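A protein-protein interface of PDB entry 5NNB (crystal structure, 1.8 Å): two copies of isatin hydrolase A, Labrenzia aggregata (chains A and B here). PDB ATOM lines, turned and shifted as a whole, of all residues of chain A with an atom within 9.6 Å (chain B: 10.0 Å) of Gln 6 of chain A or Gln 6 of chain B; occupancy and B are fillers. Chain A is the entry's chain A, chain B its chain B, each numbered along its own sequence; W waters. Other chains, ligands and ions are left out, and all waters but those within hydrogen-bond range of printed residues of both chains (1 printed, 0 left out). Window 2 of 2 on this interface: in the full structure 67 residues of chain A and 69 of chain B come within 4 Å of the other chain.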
ATOM      1  N   SER A   2      24.576 -13.341  -5.819  1.00  0.00           N
ATOM      2  CA  SER A   2      24.617 -13.188  -4.369  1.00  0.00           C
ATOM      3  C   SER A   2      25.086 -11.789  -3.990  1.00  0.00           C
ATOM      4  O   SER A   2      24.277 -10.889  -3.766  1.00  0.00           O
ATOM      5  CB  SER A   2      25.535 -14.234  -3.737  1.00  0.00           C
ATOM      6  OG  SER A   2      26.889 -14.007  -4.099  1.00  0.00           O
ATOM      7  N   SER A   3      26.400 -11.609  -3.922  1.00  0.00           N
ATOM      8  CA  SER A   3      26.958 -10.313  -3.558  1.00  0.00           C
ATOM      9  C   SER A   3      26.766  -9.309  -4.700  1.00  0.00           C
ATOM     10  O   SER A   3      26.620  -8.113  -4.457  1.00  0.00           O
ATOM     11  CB  SER A   3      28.439 -10.442  -3.194  1.00  0.00           C
ATOM     12  OG  SER A   3      29.218 -10.789  -4.319  1.00  0.00           O
ATOM     13  N   LEU A   4      26.772  -9.796  -5.942  1.00  0.00           N
ATOM     14  CA  LEU A   4      26.541  -8.918  -7.083  1.00  0.00           C
ATOM     15  C   LEU A   4      25.069  -8.475  -7.136  1.00  0.00           C
ATOM     16  O   LEU A   4      24.768  -7.336  -7.506  1.00  0.00           O
ATOM     17  CB  LEU A   4      26.946  -9.601  -8.390  1.00  0.00           C
ATOM     18  CG  LEU A   4      28.452  -9.799  -8.579  1.00  0.00           C
ATOM     19  CD1 LEU A   4      28.747 -10.457  -9.935  1.00  0.00           C
ATOM     20  CD2 LEU A   4      29.189  -8.473  -8.443  1.00  0.00           C
ATOM     21  N   ASN A   5      24.165  -9.377  -6.772  1.00  0.00           N
ATOM     22  CA  ASN A   5      22.744  -9.042  -6.722  1.00  0.00           C
ATOM     23  C   ASN A   5      22.509  -7.927  -5.715  1.00  0.00           C
ATOM     24  O   ASN A   5      21.712  -7.019  -5.944  1.00  0.00           O
ATOM     25  CB  ASN A   5      21.902 -10.263  -6.345  1.00  0.00           C
ATOM     26  CG  ASN A   5      21.888 -11.324  -7.428  1.00  0.00           C
ATOM     27  OD1 ASN A   5      22.082 -11.033  -8.612  1.00  0.00           O
ATOM     28  ND2 ASN A   5      21.661 -12.570  -7.025  1.00  0.00           N
ATOM     29  N   GLN A   6      23.241  -7.976  -4.610  1.00  0.00           N
ATOM     30  CA  GLN A   6      23.095  -6.945  -3.590  1.00  0.00           C
ATOM     31  C   GLN A   6      23.716  -5.634  -4.057  1.00  0.00           C
ATOM     32  O   GLN A   6      23.181  -4.564  -3.781  1.00  0.00           O
ATOM     33  CB  GLN A   6      23.703  -7.425  -2.274  1.00  0.00           C
ATOM     34  CG  GLN A   6      22.985  -8.662  -1.753  1.00  0.00           C
ATOM     35  CD  GLN A   6      23.660  -9.278  -0.563  1.00  0.00           C
ATOM     36  OE1 GLN A   6      23.009  -9.863   0.299  1.00  0.00           O
ATOM     37  NE2 GLN A   6      24.972  -9.136  -0.491  1.00  0.00           N
ATOM     38  N   LEU A   7      24.810  -5.717  -4.815  1.00  0.00           N
ATOM     39  CA  LEU A   7      25.417  -4.521  -5.386  1.00  0.00           C
ATOM     40  C   LEU A   7      24.472  -3.831  -6.365  1.00  0.00           C
ATOM     41  O   LEU A   7      24.329  -2.610  -6.348  1.00  0.00           O
ATOM     42  CB  LEU A   7      26.731  -4.855  -6.108  1.00  0.00           C
ATOM     43  CG  LEU A   7      27.388  -3.663  -6.809  1.00  0.00           C
ATOM     44  CD1 LEU A   7      27.821  -2.609  -5.792  1.00  0.00           C
ATOM     45  CD2 LEU A   7      28.557  -4.076  -7.714  1.00  0.00           C
ATOM     46  N   VAL A   8      23.831  -4.623  -7.216  1.00  0.00           N
ATOM     47  CA  VAL A   8      22.892  -4.097  -8.195  1.00  0.00           C
ATOM     48  C   VAL A   8      21.740  -3.376  -7.491  1.00  0.00           C
ATOM     49  O   VAL A   8      21.344  -2.267  -7.863  1.00  0.00           O
ATOM     50  CB  VAL A   8      22.324  -5.231  -9.070  1.00  0.00           C
ATOM     51  CG1 VAL A   8      21.117  -4.749  -9.863  1.00  0.00           C
ATOM     52  CG2 VAL A   8      23.413  -5.788  -9.985  1.00  0.00           C
ATOM     53  N   SER A   9      21.238  -4.022  -6.451  1.00  0.00           N
ATOM     54  CA  SER A   9      20.128  -3.492  -5.666  1.00  0.00           C
ATOM     55  C   SER A   9      20.502  -2.186  -4.982  1.00  0.00           C
ATOM     56  O   SER A   9      19.708  -1.239  -4.908  1.00  0.00           O
ATOM     57  CB  SER A   9      19.711  -4.520  -4.619  1.00  0.00           C
ATOM     58  OG  SER A   9      18.802  -3.953  -3.703  1.00  0.00           O
ATOM     59  N   GLY A  10      21.725  -2.147  -4.476  1.00  0.00           N
ATOM     60  CA  GLY A  10      22.230  -0.951  -3.839  1.00  0.00           C
ATOM     61  C   GLY A  10      22.414   0.183  -4.818  1.00  0.00           C
ATOM     62  O   GLY A  10      22.048   1.322  -4.525  1.00  0.00           O
ATOM     63  N   LEU A  11      22.982  -0.124  -5.986  1.00  0.00           N
ATOM     64  CA  LEU A  11      23.192   0.897  -7.000  1.00  0.00           C
ATOM     65  C   LEU A  11      21.854   1.447  -7.501  1.00  0.00           C
ATOM     66  O   LEU A  11      21.709   2.653  -7.716  1.00  0.00           O
ATOM     67  CB  LEU A  11      24.010   0.340  -8.171  1.00  0.00           C
ATOM     68  CG  LEU A  11      25.493   0.115  -7.886  1.00  0.00           C
ATOM     69  CD1 LEU A  11      26.154  -0.640  -9.038  1.00  0.00           C
ATOM     70  CD2 LEU A  11      26.193   1.443  -7.640  1.00  0.00           C
ATOM     71  N   ALA A  12      20.877   0.565  -7.655  1.00  0.00           N
ATOM     72  CA  ALA A  12      19.580   0.970  -8.176  1.00  0.00           C
ATOM     73  C   ALA A  12      18.838   1.856  -7.181  1.00  0.00           C
ATOM     74  O   ALA A  12      18.193   2.842  -7.549  1.00  0.00           O
ATOM     75  CB  ALA A  12      18.748  -0.248  -8.504  1.00  0.00           C
ATOM     76  N   SER A  13      18.955   1.511  -5.910  1.00  0.00           N
ATOM     77  CA  SER A  13      18.196   2.214  -4.885  1.00  0.00           C
ATOM     78  C   SER A  13      18.928   3.445  -4.372  1.00  0.00           C
ATOM     79  O   SER A  13      18.317   4.351  -3.806  1.00  0.00           O
ATOM     80  CB  SER A  13      17.907   1.265  -3.722  1.00  0.00           C
ATOM     81  OG  SER A  13      19.101   0.929  -3.034  1.00  0.00           O
ATOM     82  N   GLY A  14      20.235   3.498  -4.594  1.00  0.00           N
ATOM     83  CA  GLY A  14      21.007   4.611  -4.066  1.00  0.00           C
ATOM     84  C   GLY A  14      21.662   4.333  -2.717  1.00  0.00           C
ATOM     85  O   GLY A  14      22.324   5.212  -2.163  1.00  0.00           O
ATOM     86  N   ALA A  15      21.465   3.130  -2.176  1.00  0.00           N
ATOM     87  CA  ALA A  15      22.152   2.707  -0.958  1.00  0.00           C
ATOM     88  C   ALA A  15      23.657   2.611  -1.239  1.00  0.00           C
ATOM     89  O   ALA A  15      24.489   2.726  -0.343  1.00  0.00           O
ATOM     90  CB  ALA A  15      21.618   1.388  -0.462  1.00  0.00           C
ATOM     91  N   VAL A  16      23.997   2.355  -2.492  1.00  0.00           N
ATOM     92  CA  VAL A  16      25.383   2.453  -2.933  1.00  0.00           C
ATOM     93  C   VAL A  16      25.461   3.604  -3.927  1.00  0.00           C
ATOM     94  O   VAL A  16      24.722   3.638  -4.915  1.00  0.00           O
ATOM     95  CB  VAL A  16      25.891   1.131  -3.571  1.00  0.00           C
ATOM     96  CG1 VAL A  16      27.306   1.300  -4.123  1.00  0.00           C
ATOM     97  CG2 VAL A  16      25.835   0.000  -2.547  1.00  0.00           C
ATOM     98  N   PRO A 102      39.281  -2.706  -2.628  1.00  0.00           N
ATOM     99  CA  PRO A 102      39.113  -1.817  -1.473  1.00  0.00           C
ATOM    100  C   PRO A 102      40.050  -0.616  -1.575  1.00  0.00           C
ATOM    101  O   PRO A 102      41.130  -0.725  -2.166  1.00  0.00           O
ATOM    102  CB  PRO A 102      39.461  -2.719  -0.291  1.00  0.00           C
ATOM    103  CG  PRO A 102      40.388  -3.735  -0.860  1.00  0.00           C
ATOM    104  CD  PRO A 102      39.878  -3.997  -2.253  1.00  0.00           C
ATOM    105  N   GLY A 231      36.078   1.607   3.673  1.00  0.00           N
ATOM    106  CA  GLY A 231      34.785   1.049   3.313  1.00  0.00           C
ATOM    107  C   GLY A 231      34.390   1.207   1.854  1.00  0.00           C
ATOM    108  O   GLY A 231      33.454   0.552   1.396  1.00  0.00           O
ATOM    109  N   VAL A 233      34.925   1.145  -2.406  1.00  0.00           N
ATOM    110  CA  VAL A 233      35.542   0.311  -3.453  1.00  0.00           C
ATOM    111  C   VAL A 233      35.939   1.169  -4.643  1.00  0.00           C
ATOM    112  O   VAL A 233      35.128   1.927  -5.174  1.00  0.00           O
ATOM    113  CB  VAL A 233      34.605  -0.815  -3.938  1.00  0.00           C
ATOM    114  CG1 VAL A 233      35.179  -1.492  -5.210  1.00  0.00           C
ATOM    115  CG2 VAL A 233      34.360  -1.818  -2.845  1.00  0.00           C
ATOM    116  N   MET A 254      32.761   3.505  -5.413  1.00  0.00           N
ATOM    117  CA  MET A 254      31.435   3.152  -4.919  1.00  0.00           C
ATOM    118  C   MET A 254      31.463   3.292  -3.403  1.00  0.00           C
ATOM    119  O   MET A 254      32.397   2.811  -2.753  1.00  0.00           O
ATOM    120  CB  MET A 254      31.054   1.735  -5.339  1.00  0.00           C
ATOM    121  CG  MET A 254      31.023   1.558  -6.847  1.00  0.00           C
ATOM    122  SD  MET A 254      30.461  -0.076  -7.341  1.00  0.00           S
ATOM    123  CE  MET A 254      31.831  -1.104  -6.812  1.00  0.00           C
ATOM    124  N   THR A 256      29.107   3.337   0.432  1.00  0.00           N
ATOM    125  CA  THR A 256      27.853   2.971   1.102  1.00  0.00           C
ATOM    126  C   THR A 256      27.266   4.168   1.824  1.00  0.00           C
ATOM    127  O   THR A 256      28.003   5.057   2.239  1.00  0.00           O
ATOM    128  CB  THR A 256      28.039   1.832   2.131  1.00  0.00           C
ATOM    129  OG1 THR A 256      28.544   0.659   1.483  1.00  0.00           O
ATOM    130  CG2 THR A 256      26.705   1.497   2.800  1.00  0.00           C
ATOM    131  N   SER B   2      27.990  -4.998   4.489  1.00  0.00           N
ATOM    132  CA  SER B   2      27.401  -4.240   3.391  1.00  0.00           C
ATOM    133  C   SER B   2      27.714  -4.920   2.072  1.00  0.00           C
ATOM    134  O   SER B   2      28.566  -5.807   2.008  1.00  0.00           O
ATOM    135  CB  SER B   2      27.921  -2.801   3.358  1.00  0.00           C
ATOM    136  OG  SER B   2      29.294  -2.758   2.990  1.00  0.00           O
ATOM    137  N   SER B   3      27.077  -4.455   1.009  1.00  0.00           N
ATOM    138  CA  SER B   3      27.277  -5.068  -0.294  1.00  0.00           C
ATOM    139  C   SER B   3      28.690  -4.794  -0.806  1.00  0.00           C
ATOM    140  O   SER B   3      29.255  -5.612  -1.533  1.00  0.00           O
ATOM    141  CB  SER B   3      26.228  -4.574  -1.294  1.00  0.00           C
ATOM    142  OG  SER B   3      26.377  -3.191  -1.572  1.00  0.00           O
ATOM    143  N   LEU B   4      29.269  -3.655  -0.426  1.00  0.00           N
ATOM    144  CA  LEU B   4      30.634  -3.351  -0.851  1.00  0.00           C
ATOM    145  C   LEU B   4      31.685  -4.207  -0.124  1.00  0.00           C
ATOM    146  O   LEU B   4      32.667  -4.637  -0.737  1.00  0.00           O
ATOM    147  CB  LEU B   4      30.925  -1.866  -0.661  1.00  0.00           C
ATOM    148  CG  LEU B   4      30.150  -0.956  -1.620  1.00  0.00           C
ATOM    149  CD1 LEU B   4      30.519   0.482  -1.366  1.00  0.00           C
ATOM    150  CD2 LEU B   4      30.364  -1.331  -3.093  1.00  0.00           C
ATOM    151  N   ASN B   5      31.485  -4.466   1.167  1.00  0.00           N
ATOM    152  CA  ASN B   5      32.411  -5.325   1.912  1.00  0.00           C
ATOM    153  C   ASN B   5      32.411  -6.768   1.389  1.00  0.00           C
ATOM    154  O   ASN B   5      33.456  -7.414   1.308  1.00  0.00           O
ATOM    155  CB  ASN B   5      32.084  -5.289   3.412  1.00  0.00           C
ATOM    156  CG  ASN B   5      32.371  -3.925   4.044  1.00  0.00           C
ATOM    157  OD1 ASN B   5      33.205  -3.161   3.550  1.00  0.00           O
ATOM    158  ND2 ASN B   5      31.672  -3.613   5.136  1.00  0.00           N
ATOM    159  N   GLN B   6      31.230  -7.256   1.025  1.00  0.00           N
ATOM    160  CA  GLN B   6      31.057  -8.606   0.489  1.00  0.00           C
ATOM    161  C   GLN B   6      31.576  -8.729  -0.953  1.00  0.00           C
ATOM    162  O   GLN B   6      32.028  -9.804  -1.363  1.00  0.00           O
ATOM    163  CB  GLN B   6      29.586  -9.003   0.613  1.00  0.00           C
ATOM    164  CG  GLN B   6      29.162  -9.021   2.091  1.00  0.00           C
ATOM    165  CD  GLN B   6      27.674  -9.185   2.316  1.00  0.00           C
ATOM    166  OE1 GLN B   6      27.246  -9.782   3.304  1.00  0.00           O
ATOM    167  NE2 GLN B   6      26.876  -8.632   1.415  1.00  0.00           N
ATOM    168  N   LEU B   7      31.479  -7.648  -1.732  1.00  0.00           N
ATOM    169  CA  LEU B   7      32.102  -7.599  -3.062  1.00  0.00           C
ATOM    170  C   LEU B   7      33.622  -7.696  -2.906  1.00  0.00           C
ATOM    171  O   LEU B   7      34.288  -8.390  -3.660  1.00  0.00           O
ATOM    172  CB  LEU B   7      31.740  -6.313  -3.822  1.00  0.00           C
ATOM    173  CG  LEU B   7      32.453  -6.110  -5.172  1.00  0.00           C
ATOM    174  CD1 LEU B   7      32.079  -7.180  -6.218  1.00  0.00           C
ATOM    175  CD2 LEU B   7      32.259  -4.705  -5.736  1.00  0.00           C
ATOM    176  N   VAL B   8      34.172  -6.977  -1.929  1.00  0.00           N
ATOM    177  CA  VAL B   8      35.618  -7.031  -1.688  1.00  0.00           C
ATOM    178  C   VAL B   8      36.046  -8.442  -1.304  1.00  0.00           C
ATOM    179  O   VAL B   8      37.073  -8.954  -1.771  1.00  0.00           O
ATOM    180  CB  VAL B   8      36.056  -6.035  -0.586  1.00  0.00           C
ATOM    181  CG1 VAL B   8      37.494  -6.310  -0.138  1.00  0.00           C
ATOM    182  CG2 VAL B   8      35.918  -4.609  -1.077  1.00  0.00           C
ATOM    183  N   SER B   9      35.272  -9.066  -0.431  1.00  0.00           N
ATOM    184  CA  SER B   9      35.586 -10.415   0.006  1.00  0.00           C
ATOM    185  C   SER B   9      35.467 -11.405  -1.153  1.00  0.00           C
ATOM    186  O   SER B   9      36.300 -12.298  -1.307  1.00  0.00           O
ATOM    187  CB  SER B   9      34.672 -10.831   1.153  1.00  0.00           C
ATOM    188  OG  SER B   9      34.893 -12.186   1.481  1.00  0.00           O
ATOM    189  N   GLY B  10      34.448 -11.228  -1.986  1.00  0.00           N
ATOM    190  CA  GLY B  10      34.257 -12.110  -3.129  1.00  0.00           C
ATOM    191  C   GLY B  10      35.372 -11.995  -4.154  1.00  0.00           C
ATOM    192  O   GLY B  10      35.855 -13.000  -4.681  1.00  0.00           O
ATOM    193  N   LEU B  11      35.783 -10.765  -4.441  1.00  0.00           N
ATOM    194  CA  LEU B  11      36.883 -10.524  -5.371  1.00  0.00           C
ATOM    195  C   LEU B  11      38.180 -11.119  -4.826  1.00  0.00           C
ATOM    196  O   LEU B  11      38.992 -11.637  -5.588  1.00  0.00           O
ATOM    197  CB  LEU B  11      37.046  -9.030  -5.635  1.00  0.00           C
ATOM    198  CG  LEU B  11      35.954  -8.404  -6.494  1.00  0.00           C
ATOM    199  CD1 LEU B  11      36.094  -6.901  -6.488  1.00  0.00           C
ATOM    200  CD2 LEU B  11      36.047  -8.950  -7.914  1.00  0.00           C
ATOM    201  N   ALA B  12      38.369 -11.043  -3.508  1.00  0.00           N
ATOM    202  CA  ALA B  12      39.579 -11.556  -2.873  1.00  0.00           C
ATOM    203  C   ALA B  12      39.657 -13.077  -2.926  1.00  0.00           C
ATOM    204  O   ALA B  12      40.734 -13.640  -3.141  1.00  0.00           O
ATOM    205  CB  ALA B  12      39.657 -11.085  -1.424  1.00  0.00           C
ATOM    206  N   SER B  13      38.518 -13.739  -2.735  1.00  0.00           N
ATOM    207  CA  SER B  13      38.481 -15.200  -2.660  1.00  0.00           C
ATOM    208  C   SER B  13      38.304 -15.878  -4.021  1.00  0.00           C
ATOM    209  O   SER B  13      38.530 -17.084  -4.158  1.00  0.00           O
ATOM    210  CB  SER B  13      37.365 -15.651  -1.721  1.00  0.00           C
ATOM    211  OG  SER B  13      36.103 -15.358  -2.284  1.00  0.00           O
ATOM    212  N   GLY B  14      37.880 -15.109  -5.017  1.00  0.00           N
ATOM    213  CA  GLY B  14      37.632 -15.651  -6.339  1.00  0.00           C
ATOM    214  C   GLY B  14      36.181 -16.039  -6.574  1.00  0.00           C
ATOM    215  O   GLY B  14      35.835 -16.538  -7.641  1.00  0.00           O
ATOM    216  N   ALA B  15      35.333 -15.832  -5.572  1.00  0.00           N
ATOM    217  CA  ALA B  15      33.897 -16.090  -5.707  1.00  0.00           C
ATOM    218  C   ALA B  15      33.269 -15.139  -6.723  1.00  0.00           C
ATOM    219  O   ALA B  15      32.287 -15.470  -7.377  1.00  0.00           O
ATOM    220  CB  ALA B  15      33.205 -15.961  -4.347  1.00  0.00           C
ATOM    221  N   VAL B  16      33.852 -13.953  -6.836  1.00  0.00           N
ATOM    222  CA  VAL B  16      33.518 -13.005  -7.885  1.00  0.00           C
ATOM    223  C   VAL B  16      34.731 -12.825  -8.801  1.00  0.00           C
ATOM    224  O   VAL B  16      35.832 -12.486  -8.350  1.00  0.00           O
ATOM    225  CB  VAL B  16      33.093 -11.636  -7.319  1.00  0.00           C
ATOM    226  CG1 VAL B  16      32.829 -10.644  -8.452  1.00  0.00           C
ATOM    227  CG2 VAL B  16      31.862 -11.788  -6.446  1.00  0.00           C
ATOM    228  N   ARG B  17      34.518 -13.071 -10.084  1.00  0.00           N
ATOM    229  CA  ARG B  17      35.570 -12.960 -11.078  1.00  0.00           C
ATOM    230  C   ARG B  17      35.331 -11.733 -11.959  1.00  0.00           C
ATOM    231  O   ARG B  17      34.190 -11.301 -12.153  1.00  0.00           O
ATOM    232  CB  ARG B  17      35.618 -14.244 -11.909  1.00  0.00           C
ATOM    233  CG  ARG B  17      36.817 -14.399 -12.816  1.00  0.00           C
ATOM    234  CD  ARG B  17      36.736 -15.723 -13.574  1.00  0.00           C
ATOM    235  NE  ARG B  17      35.619 -15.740 -14.519  1.00  0.00           N
ATOM    236  CZ  ARG B  17      35.261 -16.797 -15.243  1.00  0.00           C
ATOM    237  NH1 ARG B  17      35.933 -17.937 -15.137  1.00  0.00           N
ATOM    238  NH2 ARG B  17      34.227 -16.714 -16.075  1.00  0.00           N
ATOM    239  N   PRO B 102      23.578  -3.634 -13.849  1.00  0.00           N
ATOM    240  CA  PRO B 102      23.217  -4.974 -14.300  1.00  0.00           C
ATOM    241  C   PRO B 102      23.286  -5.066 -15.819  1.00  0.00           C
ATOM    242  O   PRO B 102      23.036  -4.087 -16.530  1.00  0.00           O
ATOM    243  CB  PRO B 102      21.775  -5.145 -13.788  1.00  0.00           C
ATOM    244  CG  PRO B 102      21.244  -3.768 -13.727  1.00  0.00           C
ATOM    245  CD  PRO B 102      22.415  -2.912 -13.295  1.00  0.00           C
ATOM    246  N   GLY B 231      22.764 -11.712 -14.255  1.00  0.00           N
ATOM    247  CA  GLY B 231      23.462 -11.765 -12.983  1.00  0.00           C
ATOM    248  C   GLY B 231      24.824 -11.092 -12.964  1.00  0.00           C
ATOM    249  O   GLY B 231      25.392 -10.866 -11.900  1.00  0.00           O
ATOM    250  N   ALA B 232      25.377 -10.791 -14.133  1.00  0.00           N
ATOM    251  CA  ALA B 232      26.666 -10.105 -14.161  1.00  0.00           C
ATOM    252  C   ALA B 232      26.482  -8.584 -14.000  1.00  0.00           C
ATOM    253  O   ALA B 232      25.400  -8.037 -14.230  1.00  0.00           O
ATOM    254  CB  ALA B 232      27.419 -10.434 -15.442  1.00  0.00           C
ATOM    255  N   VAL B 233      27.539  -7.911 -13.570  1.00  0.00           N
ATOM    256  CA  VAL B 233      27.536  -6.469 -13.453  1.00  0.00           C
ATOM    257  C   VAL B 233      28.532  -5.844 -14.410  1.00  0.00           C
ATOM    258  O   VAL B 233      29.729  -6.167 -14.377  1.00  0.00           O
ATOM    259  CB  VAL B 233      27.884  -6.023 -12.004  1.00  0.00           C
ATOM    260  CG1 VAL B 233      28.082  -4.530 -11.960  1.00  0.00           C
ATOM    261  CG2 VAL B 233      26.789  -6.470 -11.031  1.00  0.00           C
ATOM    262  N   MET B 254      31.780  -8.098 -13.970  1.00  0.00           N
ATOM    263  CA  MET B 254      31.964  -8.905 -12.773  1.00  0.00           C
ATOM    264  C   MET B 254      30.949 -10.038 -12.783  1.00  0.00           C
ATOM    265  O   MET B 254      29.773  -9.807 -13.042  1.00  0.00           O
ATOM    266  CB  MET B 254      31.824  -8.039 -11.511  1.00  0.00           C
ATOM    267  CG  MET B 254      32.860  -6.922 -11.468  1.00  0.00           C
ATOM    268  SD  MET B 254      32.870  -6.005  -9.912  1.00  0.00           S
ATOM    269  CE  MET B 254      31.294  -5.156  -9.972  1.00  0.00           C
ATOM    270  N   THR B 256      29.664 -14.024 -10.989  1.00  0.00           N
ATOM    271  CA  THR B 256      29.734 -14.996  -9.898  1.00  0.00           C
ATOM    272  C   THR B 256      30.084 -16.385 -10.437  1.00  0.00           C
ATOM    273  O   THR B 256      31.150 -16.935 -10.139  1.00  0.00           O
ATOM    274  CB  THR B 256      28.410 -15.093  -9.115  1.00  0.00           C
ATOM    275  OG1 THR B 256      27.349 -15.409 -10.019  1.00  0.00           O
ATOM    276  CG2 THR B 256      28.095 -13.782  -8.402  1.00  0.00           C
HETATM  277  O   HOH W   1      31.403  -0.595   3.174  1.00  0.00           O
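NE2 of Gln 6 of chain B lies close to NE2 of Gln 6 of chain A (2.7 Å).
The backbone carbonyl oxygen (O) of Gly 10 of chain A is in hydrogen-bond range of the backbone NH (N) of Val 16 of chain A, 3.0 Å away.
The backbone NH of Met 254 of chain A sits at hydrogen-bond distance from the backbone carbonyl oxygen of Val 233 of chain A (2.9 Å).
The side-chain hydroxyl of Ser 2 of chain B sits at hydrogen-bond distance from the side-chain amide nitrogen of Asn 5 of chain B (3.3 Å).
The backbone carbonyl oxygen (O) of Ser 2 of chain B lies close to the side-chain amide nitrogen (NE2) of Gln 6 of chain B (3.3 Å).
The backbone carbonyl oxygen (O) of Gly 10 of chain B is in hydrogen-bond range of the backbone NH (N) of Val 16 of chain B, 3.1 Å away.
The backbone carbonyl oxygen (O) of Val 233 of chain B sits at hydrogen-bond distance from the backbone NH (N) of Met 254 of chain B (2.8 Å).
Among the printed residues, pairs that only touch across the chains: Met 254 of chain A with Leu 4 of chain B, Leu 4 of chain A with Met 254 of chain B, Val 16 of chain A with Ser 3 of chain B, Thr 256 of chain A with Leu 4 of chain B, Ser 3 of chain A with Val 16 of chain B, Val 8 of chain A with Val 233 of chain B, Val 233 of chain A with Val 8 of chain B, Leu 7 of chain A with Met 254 of chain B, Leu 4 of chain A with Thr 256 of chain B, Met 254 of chain A with Leu 7 of chain B, Thr 256 of chain A with Ser 2 of chain B, Leu 4 of chain A with Leu 7 of chain B, Gln 6 of chain A with Ser 3 of chain B, Val 233 of chain A with Leu 4 of chain B, Leu 4 of chain A with Gly 231 of chain B, Leu 7 of chain A with Leu 4 of chain B, Pro 102 of chain A with Val 8 of chain B, Leu 7 of chain A with Ser 3 of chain B and Val 8 of chain A with Pro 102 of chain B.
Ser 3 of chain A touches just one residue of chain B: Val 16.
Gln 6 of chain A touches just these residues of chain B: Ser 3 and Gln 6.
Printed residues of chain B within 4 Å of Val 8 of chain A: Pro 102 and Val 233.
No residue of chain B comes within 4 Å of Ser 9 of chain A.
Gly 10 of chain A touches none of the printed residues of chain B.
Gly 14 of chain A touches none of the printed residues of chain B.
Printed residues of chain B within 4 Å of Val 233 of chain A: Leu 4 and Val 8.
Ser 3 of chain B touches just these residues of chain A: Gln 6, Leu 7 and Val 16.
Asn 5 of chain B touches none of the printed residues of chain A.
Gln 6 of chain B touches one residue of chain A.
Of the printed residues of chain A, Val 16 of chain B touches Ser 3 (3.5 Å).
The nearest residue of chain B that does not touch Gln 6 of chain A is Ser 2 of chain B (5.5 Å).
The nearest printed residue of chain A that does not touch Met 254 of chain B is Met 254 of chain A (5.2 Å).
Hydrophobic or aromatic side chains of chain B that line the printed part of chain A: Leu 4, Leu 7, Val 8, Val 16, Pro 102, Val 233 and Met 254.
Printed residues of chain A that touch a printed residue of chain B: Ser 3, Leu 4, Gln 6, Leu 7, Val 8, Val 16, Pro 102, Val 233, Met 254 and Thr 256.
Among the printed residues, 20 pairs touch across the chains.
Leu 4 of chain A touches Met 254 of chain B, and with the chains exchanged Met 254 of chain A touches Leu 4 of chain B.
Leu 4 of chain A touches Thr 256 of chain B, and with the chains exchanged Thr 256 of chain A touches Leu 4 of chain B.
Gln 6 of chain A touches Ser 3 of chain B, but with the chains exchanged Ser 3 of chain A does not touch Gln 6 of chain B (4.1 Å).
Thr 256 of chain A touches Ser 2 of chain B, but with the chains exchanged Ser 2 of chain A does not touch Thr 256 of chain B (4.4 Å).
20 positions are printed for both chains.
Water W1 lies within hydrogen-bond range of O of Gly 231 of chain A (2.9 Å), OG of Ser 2 of chain B (3.0 Å) and OD1 of Asn 5 of chain B (3.2 Å).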
